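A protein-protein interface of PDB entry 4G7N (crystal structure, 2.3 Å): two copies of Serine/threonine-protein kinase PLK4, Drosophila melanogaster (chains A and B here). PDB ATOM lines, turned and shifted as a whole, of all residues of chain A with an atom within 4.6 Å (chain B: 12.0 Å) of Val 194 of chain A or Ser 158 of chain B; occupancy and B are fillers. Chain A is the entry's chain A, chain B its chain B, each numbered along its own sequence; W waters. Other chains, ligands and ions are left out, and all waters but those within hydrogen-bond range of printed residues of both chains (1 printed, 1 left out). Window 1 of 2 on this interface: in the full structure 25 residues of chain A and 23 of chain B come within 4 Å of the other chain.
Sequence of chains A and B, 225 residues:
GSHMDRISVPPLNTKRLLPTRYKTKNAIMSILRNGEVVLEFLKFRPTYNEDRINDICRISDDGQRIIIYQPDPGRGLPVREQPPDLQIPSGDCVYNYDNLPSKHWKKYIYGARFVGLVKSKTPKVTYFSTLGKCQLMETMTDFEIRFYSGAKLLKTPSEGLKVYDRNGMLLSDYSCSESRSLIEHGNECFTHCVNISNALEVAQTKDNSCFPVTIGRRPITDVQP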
ATOM      1  N   LEU A 136      -3.215  22.268  24.189  1.00  0.00           N
ATOM      2  CA  LEU A 136      -4.207  23.329  24.232  1.00  0.00           C
ATOM      3  C   LEU A 136      -3.679  24.398  25.182  1.00  0.00           C
ATOM      4  O   LEU A 136      -3.281  24.093  26.307  1.00  0.00           O
ATOM      5  CB  LEU A 136      -5.518  22.768  24.760  1.00  0.00           C
ATOM      6  CG  LEU A 136      -6.645  23.744  25.061  1.00  0.00           C
ATOM      7  CD1 LEU A 136      -7.176  24.371  23.780  1.00  0.00           C
ATOM      8  CD2 LEU A 136      -7.736  23.017  25.796  1.00  0.00           C
ATOM      9  N   MET A 140      -7.354  28.726  25.723  1.00  0.00           N
ATOM     10  CA  MET A 140      -8.433  27.780  25.382  1.00  0.00           C
ATOM     11  C   MET A 140      -8.792  27.738  23.880  1.00  0.00           C
ATOM     12  O   MET A 140      -9.689  26.998  23.482  1.00  0.00           O
ATOM     13  CB  MET A 140      -9.689  28.038  26.231  1.00  0.00           C
ATOM     14  CG  MET A 140      -9.484  27.741  27.722  1.00  0.00           C
ATOM     15  SD  MET A 140      -9.089  25.984  28.020  1.00  0.00           S
ATOM     16  CE  MET A 140     -10.676  25.174  27.737  1.00  0.00           C
ATOM     17  N   PHE A 190      -8.706  17.982  19.906  1.00  0.00           N
ATOM     18  CA  PHE A 190      -9.052  19.290  20.440  1.00  0.00           C
ATOM     19  C   PHE A 190     -10.273  19.166  21.345  1.00  0.00           C
ATOM     20  O   PHE A 190     -10.326  19.730  22.428  1.00  0.00           O
ATOM     21  CB  PHE A 190      -9.299  20.284  19.310  1.00  0.00           C
ATOM     22  CG  PHE A 190      -9.862  21.592  19.775  1.00  0.00           C
ATOM     23  CD1 PHE A 190      -9.042  22.548  20.356  1.00  0.00           C
ATOM     24  CD2 PHE A 190     -11.212  21.871  19.624  1.00  0.00           C
ATOM     25  CE1 PHE A 190      -9.553  23.752  20.769  1.00  0.00           C
ATOM     26  CE2 PHE A 190     -11.731  23.076  20.036  1.00  0.00           C
ATOM     27  CZ  PHE A 190     -10.895  24.019  20.612  1.00  0.00           C
ATOM     28  N   THR A 191     -11.243  18.387  20.903  1.00  0.00           N
ATOM     29  CA  THR A 191     -12.412  18.116  21.711  1.00  0.00           C
ATOM     30  C   THR A 191     -12.018  17.470  23.046  1.00  0.00           C
ATOM     31  O   THR A 191     -12.574  17.800  24.092  1.00  0.00           O
ATOM     32  CB  THR A 191     -13.411  17.243  20.927  1.00  0.00           C
ATOM     33  OG1 THR A 191     -13.681  17.872  19.667  1.00  0.00           O
ATOM     34  CG2 THR A 191     -14.712  17.090  21.683  1.00  0.00           C
ATOM     35  N   HIS A 192     -11.050  16.561  23.016  1.00  0.00           N
ATOM     36  CA  HIS A 192     -10.612  15.870  24.236  1.00  0.00           C
ATOM     37  C   HIS A 192      -9.891  16.807  25.207  1.00  0.00           C
ATOM     38  O   HIS A 192     -10.155  16.788  26.398  1.00  0.00           O
ATOM     39  CB  HIS A 192      -9.709  14.688  23.867  1.00  0.00           C
ATOM     40  CG  HIS A 192      -9.261  13.868  25.039  1.00  0.00           C
ATOM     41  ND1 HIS A 192     -10.142  13.281  25.917  1.00  0.00           N
ATOM     42  CD2 HIS A 192      -8.019  13.521  25.458  1.00  0.00           C
ATOM     43  CE1 HIS A 192      -9.465  12.603  26.831  1.00  0.00           C
ATOM     44  NE2 HIS A 192      -8.175  12.730  26.572  1.00  0.00           N
ATOM     45  N   CYS A 193      -8.982  17.638  24.702  1.00  0.00           N
ATOM     46  CA  CYS A 193      -8.261  18.538  25.590  1.00  0.00           C
ATOM     47  C   CYS A 193      -9.216  19.538  26.248  1.00  0.00           C
ATOM     48  O   CYS A 193      -9.029  19.932  27.398  1.00  0.00           O
ATOM     49  CB  CYS A 193      -7.149  19.282  24.850  1.00  0.00           C
ATOM     50  SG  CYS A 193      -5.793  18.213  24.277  1.00  0.00           S
ATOM     51  N   VAL A 194     -10.232  19.960  25.510  1.00  0.00           N
ATOM     52  CA  VAL A 194     -11.224  20.848  26.087  1.00  0.00           C
ATOM     53  C   VAL A 194     -12.011  20.107  27.170  1.00  0.00           C
ATOM     54  O   VAL A 194     -12.205  20.646  28.254  1.00  0.00           O
ATOM     55  CB  VAL A 194     -12.151  21.437  25.027  1.00  0.00           C
ATOM     56  CG1 VAL A 194     -13.326  22.193  25.695  1.00  0.00           C
ATOM     57  CG2 VAL A 194     -11.358  22.357  24.129  1.00  0.00           C
ATOM     58  N   ASN A 195     -12.441  18.874  26.893  1.00  0.00           N
ATOM     59  CA  ASN A 195     -13.121  18.080  27.918  1.00  0.00           C
ATOM     60  C   ASN A 195     -12.269  17.899  29.155  1.00  0.00           C
ATOM     61  O   ASN A 195     -12.791  17.869  30.262  1.00  0.00           O
ATOM     62  CB  ASN A 195     -13.505  16.689  27.407  1.00  0.00           C
ATOM     63  CG  ASN A 195     -14.532  16.743  26.320  1.00  0.00           C
ATOM     64  OD1 ASN A 195     -15.183  17.770  26.131  1.00  0.00           O
ATOM     65  ND2 ASN A 195     -14.682  15.643  25.579  1.00  0.00           N
ATOM     66  N   ILE A 196     -10.958  17.741  28.970  1.00  0.00           N
ATOM     67  CA  ILE A 196     -10.071  17.590  30.118  1.00  0.00           C
ATOM     68  C   ILE A 196     -10.033  18.868  30.937  1.00  0.00           C
ATOM     69  O   ILE A 196     -10.116  18.827  32.155  1.00  0.00           O
ATOM     70  CB  ILE A 196      -8.645  17.199  29.706  1.00  0.00           C
ATOM     71  CG1 ILE A 196      -8.589  15.709  29.367  1.00  0.00           C
ATOM     72  CG2 ILE A 196      -7.668  17.505  30.830  1.00  0.00           C
ATOM     73  CD1 ILE A 196      -7.751  15.409  28.160  1.00  0.00           C
ATOM     74  N   SER A 197      -9.916  20.001  30.254  1.00  0.00           N
ATOM     75  CA  SER A 197      -9.922  21.288  30.927  1.00  0.00           C
ATOM     76  C   SER A 197     -11.193  21.457  31.727  1.00  0.00           C
ATOM     77  O   SER A 197     -11.153  21.817  32.897  1.00  0.00           O
ATOM     78  CB  SER A 197      -9.822  22.423  29.925  1.00  0.00           C
ATOM     79  OG  SER A 197      -9.510  23.614  30.610  1.00  0.00           O
ATOM     80  N   ASN A 198     -12.324  21.200  31.081  1.00  0.00           N
ATOM     81  CA  ASN A 198     -13.624  21.268  31.745  1.00  0.00           C
ATOM     82  C   ASN A 198     -13.761  20.329  32.945  1.00  0.00           C
ATOM     83  O   ASN A 198     -14.254  20.745  33.996  1.00  0.00           O
ATOM     84  CB  ASN A 198     -14.762  21.031  30.741  1.00  0.00           C
ATOM     85  CG  ASN A 198     -14.852  22.130  29.679  1.00  0.00           C
ATOM     86  OD1 ASN A 198     -14.344  23.237  29.867  1.00  0.00           O
ATOM     87  ND2 ASN A 198     -15.502  21.825  28.566  1.00  0.00           N
ATOM     88  N   GLY B 116     -19.089  38.595  12.581  1.00  0.00           N
ATOM     89  CA  GLY B 116     -18.679  37.238  12.907  1.00  0.00           C
ATOM     90  C   GLY B 116     -19.852  36.291  13.148  1.00  0.00           C
ATOM     91  O   GLY B 116     -19.853  35.135  12.695  1.00  0.00           O
ATOM     92  N   SER B 120     -21.117  33.118  10.927  1.00  0.00           N
ATOM     93  CA  SER B 120     -21.116  31.788  11.528  1.00  0.00           C
ATOM     94  C   SER B 120     -22.425  31.056  11.271  1.00  0.00           C
ATOM     95  O   SER B 120     -22.546  29.876  11.579  1.00  0.00           O
ATOM     96  CB  SER B 120     -20.846  31.862  13.047  1.00  0.00           C
ATOM     97  OG  SER B 120     -21.932  32.435  13.754  1.00  0.00           O
ATOM     98  N   THR B 139     -17.471  31.337   7.961  1.00  0.00           N
ATOM     99  CA  THR B 139     -16.284  31.442   8.795  1.00  0.00           C
ATOM    100  C   THR B 139     -15.238  30.377   8.487  1.00  0.00           C
ATOM    101  O   THR B 139     -14.100  30.501   8.943  1.00  0.00           O
ATOM    102  CB  THR B 139     -16.617  31.325  10.284  1.00  0.00           C
ATOM    103  OG1 THR B 139     -17.335  30.108  10.502  1.00  0.00           O
ATOM    104  CG2 THR B 139     -17.459  32.520  10.768  1.00  0.00           C
ATOM    105  N   MET B 140     -15.624  29.344   7.729  1.00  0.00           N
ATOM    106  CA  MET B 140     -14.791  28.145   7.474  1.00  0.00           C
ATOM    107  C   MET B 140     -14.530  27.264   8.702  1.00  0.00           C
ATOM    108  O   MET B 140     -13.887  26.222   8.588  1.00  0.00           O
ATOM    109  CB  MET B 140     -13.453  28.506   6.809  1.00  0.00           C
ATOM    110  CG  MET B 140     -13.607  29.122   5.428  1.00  0.00           C
ATOM    111  SD  MET B 140     -14.298  27.969   4.223  1.00  0.00           S
ATOM    112  CE  MET B 140     -12.899  26.860   4.038  1.00  0.00           C
ATOM    113  N   THR B 141     -15.023  27.671   9.868  1.00  0.00           N
ATOM    114  CA  THR B 141     -14.837  26.884  11.091  1.00  0.00           C
ATOM    115  C   THR B 141     -16.154  26.321  11.629  1.00  0.00           C
ATOM    116  O   THR B 141     -16.178  25.242  12.199  1.00  0.00           O
ATOM    117  CB  THR B 141     -14.159  27.708  12.210  1.00  0.00           C
ATOM    118  OG1 THR B 141     -14.929  28.886  12.443  1.00  0.00           O
ATOM    119  CG2 THR B 141     -12.741  28.133  11.815  1.00  0.00           C
ATOM    120  N   ASP B 142     -17.248  27.051  11.456  1.00  0.00           N
ATOM    121  CA  ASP B 142     -18.549  26.581  11.926  1.00  0.00           C
ATOM    122  C   ASP B 142     -19.145  25.666  10.892  1.00  0.00           C
ATOM    123  O   ASP B 142     -19.066  25.935   9.699  1.00  0.00           O
ATOM    124  CB  ASP B 142     -19.487  27.752  12.180  1.00  0.00           C
ATOM    125  CG  ASP B 142     -19.142  28.507  13.450  1.00  0.00           C
ATOM    126  OD1 ASP B 142     -18.227  29.356  13.425  1.00  0.00           O
ATOM    127  OD2 ASP B 142     -19.780  28.231  14.482  1.00  0.00           O
ATOM    128  N   PHE B 143     -19.764  24.594  11.360  1.00  0.00           N
ATOM    129  CA  PHE B 143     -20.142  23.495  10.506  1.00  0.00           C
ATOM    130  C   PHE B 143     -21.138  22.608  11.219  1.00  0.00           C
ATOM    131  O   PHE B 143     -21.040  22.378  12.422  1.00  0.00           O
ATOM    132  CB  PHE B 143     -18.901  22.679  10.154  1.00  0.00           C
ATOM    133  CG  PHE B 143     -19.202  21.416   9.395  1.00  0.00           C
ATOM    134  CD1 PHE B 143     -19.474  21.451   8.040  1.00  0.00           C
ATOM    135  CD2 PHE B 143     -19.216  20.191  10.040  1.00  0.00           C
ATOM    136  CE1 PHE B 143     -19.745  20.289   7.343  1.00  0.00           C
ATOM    137  CE2 PHE B 143     -19.489  19.021   9.342  1.00  0.00           C
ATOM    138  CZ  PHE B 143     -19.751  19.075   7.996  1.00  0.00           C
ATOM    139  N   LEU B 154     -22.579  19.239  15.514  1.00  0.00           N
ATOM    140  CA  LEU B 154     -22.216  20.647  15.566  1.00  0.00           C
ATOM    141  C   LEU B 154     -20.712  20.768  15.703  1.00  0.00           C
ATOM    142  O   LEU B 154     -20.123  20.163  16.609  1.00  0.00           O
ATOM    143  CB  LEU B 154     -22.843  21.329  16.791  1.00  0.00           C
ATOM    144  CG  LEU B 154     -24.300  21.786  16.787  1.00  0.00           C
ATOM    145  CD1 LEU B 154     -24.448  23.080  17.608  1.00  0.00           C
ATOM    146  CD2 LEU B 154     -24.796  22.021  15.379  1.00  0.00           C
ATOM    147  N   LYS B 155     -20.080  21.545  14.829  1.00  0.00           N
ATOM    148  CA  LYS B 155     -18.666  21.852  15.016  1.00  0.00           C
ATOM    149  C   LYS B 155     -18.547  23.348  15.164  1.00  0.00           C
ATOM    150  O   LYS B 155     -19.108  24.091  14.368  1.00  0.00           O
ATOM    151  CB  LYS B 155     -17.820  21.353  13.851  1.00  0.00           C
ATOM    152  CG  LYS B 155     -16.403  21.924  13.835  1.00  0.00           C
ATOM    153  CD  LYS B 155     -15.663  21.542  12.558  1.00  0.00           C
ATOM    154  CE  LYS B 155     -14.174  21.902  12.608  1.00  0.00           C
ATOM    155  NZ  LYS B 155     -13.899  23.356  12.707  1.00  0.00           N
ATOM    156  N   THR B 156     -17.842  23.780  16.207  1.00  0.00           N
ATOM    157  CA  THR B 156     -17.612  25.198  16.489  1.00  0.00           C
ATOM    158  C   THR B 156     -16.167  25.348  16.890  1.00  0.00           C
ATOM    159  O   THR B 156     -15.544  24.376  17.308  1.00  0.00           O
ATOM    160  CB  THR B 156     -18.411  25.657  17.706  1.00  0.00           C
ATOM    161  OG1 THR B 156     -17.976  24.911  18.850  1.00  0.00           O
ATOM    162  CG2 THR B 156     -19.899  25.433  17.499  1.00  0.00           C
ATOM    163  N   PRO B 157     -15.637  26.572  16.818  1.00  0.00           N
ATOM    164  CA  PRO B 157     -14.225  26.836  17.138  1.00  0.00           C
ATOM    165  C   PRO B 157     -13.868  26.654  18.617  1.00  0.00           C
ATOM    166  O   PRO B 157     -12.694  26.465  18.919  1.00  0.00           O
ATOM    167  CB  PRO B 157     -14.043  28.313  16.747  1.00  0.00           C
ATOM    168  CG  PRO B 157     -15.218  28.636  15.857  1.00  0.00           C
ATOM    169  CD  PRO B 157     -16.337  27.792  16.388  1.00  0.00           C
ATOM    170  N   SER B 158     -14.838  26.707  19.525  1.00  0.00           N
ATOM    171  CA  SER B 158     -14.499  26.620  20.947  1.00  0.00           C
ATOM    172  C   SER B 158     -14.692  25.232  21.585  1.00  0.00           C
ATOM    173  O   SER B 158     -14.000  24.894  22.539  1.00  0.00           O
ATOM    174  CB  SER B 158     -15.243  27.692  21.750  1.00  0.00           C
ATOM    175  OG  SER B 158     -16.616  27.371  21.877  1.00  0.00           O
ATOM    176  N   GLU B 159     -15.609  24.424  21.063  1.00  0.00           N
ATOM    177  CA  GLU B 159     -15.892  23.125  21.685  1.00  0.00           C
ATOM    178  C   GLU B 159     -15.493  21.905  20.859  1.00  0.00           C
ATOM    179  O   GLU B 159     -15.347  20.818  21.411  1.00  0.00           O
ATOM    180  CB  GLU B 159     -17.378  22.990  22.012  1.00  0.00           C
ATOM    181  CG  GLU B 159     -17.972  24.140  22.802  1.00  0.00           C
ATOM    182  CD  GLU B 159     -19.488  24.197  22.667  1.00  0.00           C
ATOM    183  OE1 GLU B 159     -19.974  25.011  21.847  1.00  0.00           O
ATOM    184  OE2 GLU B 159     -20.186  23.424  23.368  1.00  0.00           O
ATOM    185  N   GLY B 160     -15.365  22.062  19.545  1.00  0.00           N
ATOM    186  CA  GLY B 160     -15.135  20.922  18.673  1.00  0.00           C
ATOM    187  C   GLY B 160     -16.426  20.245  18.237  1.00  0.00           C
ATOM    188  O   GLY B 160     -17.467  20.881  18.184  1.00  0.00           O
ATOM    189  N   LEU B 161     -16.372  18.952  17.940  1.00  0.00           N
ATOM    190  CA  LEU B 161     -17.555  18.233  17.462  1.00  0.00           C
ATOM    191  C   LEU B 161     -18.434  17.644  18.565  1.00  0.00           C
ATOM    192  O   LEU B 161     -17.951  16.928  19.434  1.00  0.00           O
ATOM    193  CB  LEU B 161     -17.138  17.128  16.509  1.00  0.00           C
ATOM    194  CG  LEU B 161     -16.222  17.596  15.384  1.00  0.00           C
ATOM    195  CD1 LEU B 161     -15.121  16.574  15.185  1.00  0.00           C
ATOM    196  CD2 LEU B 161     -17.013  17.807  14.106  1.00  0.00           C
ATOM    197  N   LYS B 162     -19.729  17.955  18.515  1.00  0.00           N
ATOM    198  CA  LYS B 162     -20.717  17.389  19.433  1.00  0.00           C
ATOM    199  C   LYS B 162     -21.842  16.837  18.580  1.00  0.00           C
ATOM    200  O   LYS B 162     -22.087  17.343  17.486  1.00  0.00           O
ATOM    201  CB  LYS B 162     -21.297  18.473  20.344  1.00  0.00           C
ATOM    202  CG  LYS B 162     -20.274  19.179  21.241  1.00  0.00           C
ATOM    203  CD  LYS B 162     -19.684  18.208  22.253  1.00  0.00           C
ATOM    204  CE  LYS B 162     -18.484  18.794  22.977  1.00  0.00           C
ATOM    205  NZ  LYS B 162     -17.688  17.704  23.610  1.00  0.00           N
ATOM    206  N   TYR B 164     -26.102  15.396  18.707  1.00  0.00           N
ATOM    207  CA  TYR B 164     -27.344  15.446  19.477  1.00  0.00           C
ATOM    208  C   TYR B 164     -28.460  14.701  18.757  1.00  0.00           C
ATOM    209  O   TYR B 164     -28.381  14.500  17.548  1.00  0.00           O
ATOM    210  CB  TYR B 164     -27.806  16.902  19.615  1.00  0.00           C
ATOM    211  CG  TYR B 164     -26.784  17.844  20.192  1.00  0.00           C
ATOM    212  CD1 TYR B 164     -26.806  18.178  21.544  1.00  0.00           C
ATOM    213  CD2 TYR B 164     -25.813  18.424  19.386  1.00  0.00           C
ATOM    214  CE1 TYR B 164     -25.876  19.052  22.077  1.00  0.00           C
ATOM    215  CE2 TYR B 164     -24.875  19.286  19.909  1.00  0.00           C
ATOM    216  CZ  TYR B 164     -24.912  19.603  21.260  1.00  0.00           C
ATOM    217  OH  TYR B 164     -23.979  20.469  21.793  1.00  0.00           O
ATOM    218  N   LEU B 170     -27.680  15.523  23.843  1.00  0.00           N
ATOM    219  CA  LEU B 170     -26.336  15.137  23.401  1.00  0.00           C
ATOM    220  C   LEU B 170     -26.016  13.653  23.583  1.00  0.00           C
ATOM    221  O   LEU B 170     -25.567  13.249  24.652  1.00  0.00           O
ATOM    222  CB  LEU B 170     -25.297  15.971  24.155  1.00  0.00           C
ATOM    223  CG  LEU B 170     -23.819  15.605  24.030  1.00  0.00           C
ATOM    224  CD1 LEU B 170     -23.336  15.797  22.604  1.00  0.00           C
ATOM    225  CD2 LEU B 170     -22.981  16.435  25.004  1.00  0.00           C
ATOM    226  N   PHE B 190     -16.922  17.431   6.784  1.00  0.00           N
ATOM    227  CA  PHE B 190     -16.298  18.719   7.032  1.00  0.00           C
ATOM    228  C   PHE B 190     -15.128  18.914   6.095  1.00  0.00           C
ATOM    229  O   PHE B 190     -14.975  19.957   5.467  1.00  0.00           O
ATOM    230  CB  PHE B 190     -15.808  18.805   8.473  1.00  0.00           C
ATOM    231  CG  PHE B 190     -14.922  19.978   8.728  1.00  0.00           C
ATOM    232  CD1 PHE B 190     -15.459  21.253   8.851  1.00  0.00           C
ATOM    233  CD2 PHE B 190     -13.547  19.814   8.836  1.00  0.00           C
ATOM    234  CE1 PHE B 190     -14.645  22.340   9.072  1.00  0.00           C
ATOM    235  CE2 PHE B 190     -12.726  20.901   9.074  1.00  0.00           C
ATOM    236  CZ  PHE B 190     -13.277  22.165   9.188  1.00  0.00           C
HETATM  237  O   HOH W   1     -12.421  26.676  23.991  1.00  0.00           O
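Of the printed residues of chain B, Val 194 of chain A touches Ser 158. Printed residues of chain A within 4 Å of Ser 158 of chain B: Phe 190 and Val 194. Phe 190 of chain A touches three residues of chain B. His 192 of chain A touches none of the printed residues of chain B. Cys 193 of chain A touches none of the printed residues of chain B. No residue of chain B comes within 4 Å of Ile 196 of chain A. No residue of chain B comes within 4 Å of Ser 197 of chain A. No residue of chain B comes within 4 Å of Asn 198 of chain A. Of the printed residues of chain A, Leu 161 of chain B touches Thr 191. Of the printed residues of chain A, Pro 157 of chain B touches Phe 190. Of the printed residues of chain A, Gly 160 of chain B touches Phe 190 and Thr 191. Printed residues of chain A within 4 Å of Lys 162 of chain B: Thr 191 and Asn 195. Phe 143 of chain B touches none of the printed residues of chain A. Asp 142 of chain B touches none of the printed residues of chain A. The nearest printed residue of chain B that does not touch Val 194 of chain A is Glu 159 of chain B (4.9 Å). The nearest printed residue of chain A that does not touch Glu 159 of chain B is Phe 190 of chain A (4.03 Å).
The side-chain amide oxygen (OD1) of Asn 195 of chain A lies close to the backbone carbonyl oxygen (O) of Thr 191 of chain A, 3.3 Å away. O of Lys 162 of chain B lies within hydrogen-bond range of N of Leu 154 of chain B, at 2.8 Å. The backbone NH (N) of Glu 159 of chain B sits at hydrogen-bond distance from the side-chain hydroxyl (OG1) of Thr 156 of chain B, 3.3 Å away.
Water W1 lies within hydrogen-bond range of O of Ser 158 of chain B (2.8 Å) and O of Met 140 of chain A (2.8 Å).
OG1 of Thr 191 of chain A is in hydrogen-bond range of N of Leu 161 of chain B, at 3.4 Å.
Among the printed residues, pairs that only touch across the chains: Phe 190 of chain A with Pro 157 of chain B (3.5 Å), Thr 191 of chain A with Gly 160 of chain B (3.5 Å), Asn 195 of chain A with Lys 162 of chain B (3.6 Å), Thr 191 of chain A with Lys 162 of chain B (3.6 Å), Phe 190 of chain A with Ser 158 of chain B (3.8 Å), Thr 191 of chain A with Glu 159 of chain B (3.8 Å), Phe 190 of chain A with Gly 160 of chain B (3.8 Å) and Val 194 of chain A with Ser 158 of chain B (3.99 Å).
Printed residues of chain B that touch a printed residue of chain A: Pro 157, Ser 158, Glu 159, Gly 160, Leu 161 and Lys 162. Of the 11 printed residues of chain A, 4 touch a printed residue of chain B. Among the printed residues, no Asp or Glu carboxylate lies within 4 Å of a Lys or Arg side-chain nitrogen of the other chain.
Positions printed for both chains: 140 and 190. Of the 9 pairs that touch across the chains among the printed residues, none has its exchanged pair printed and touching as well.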
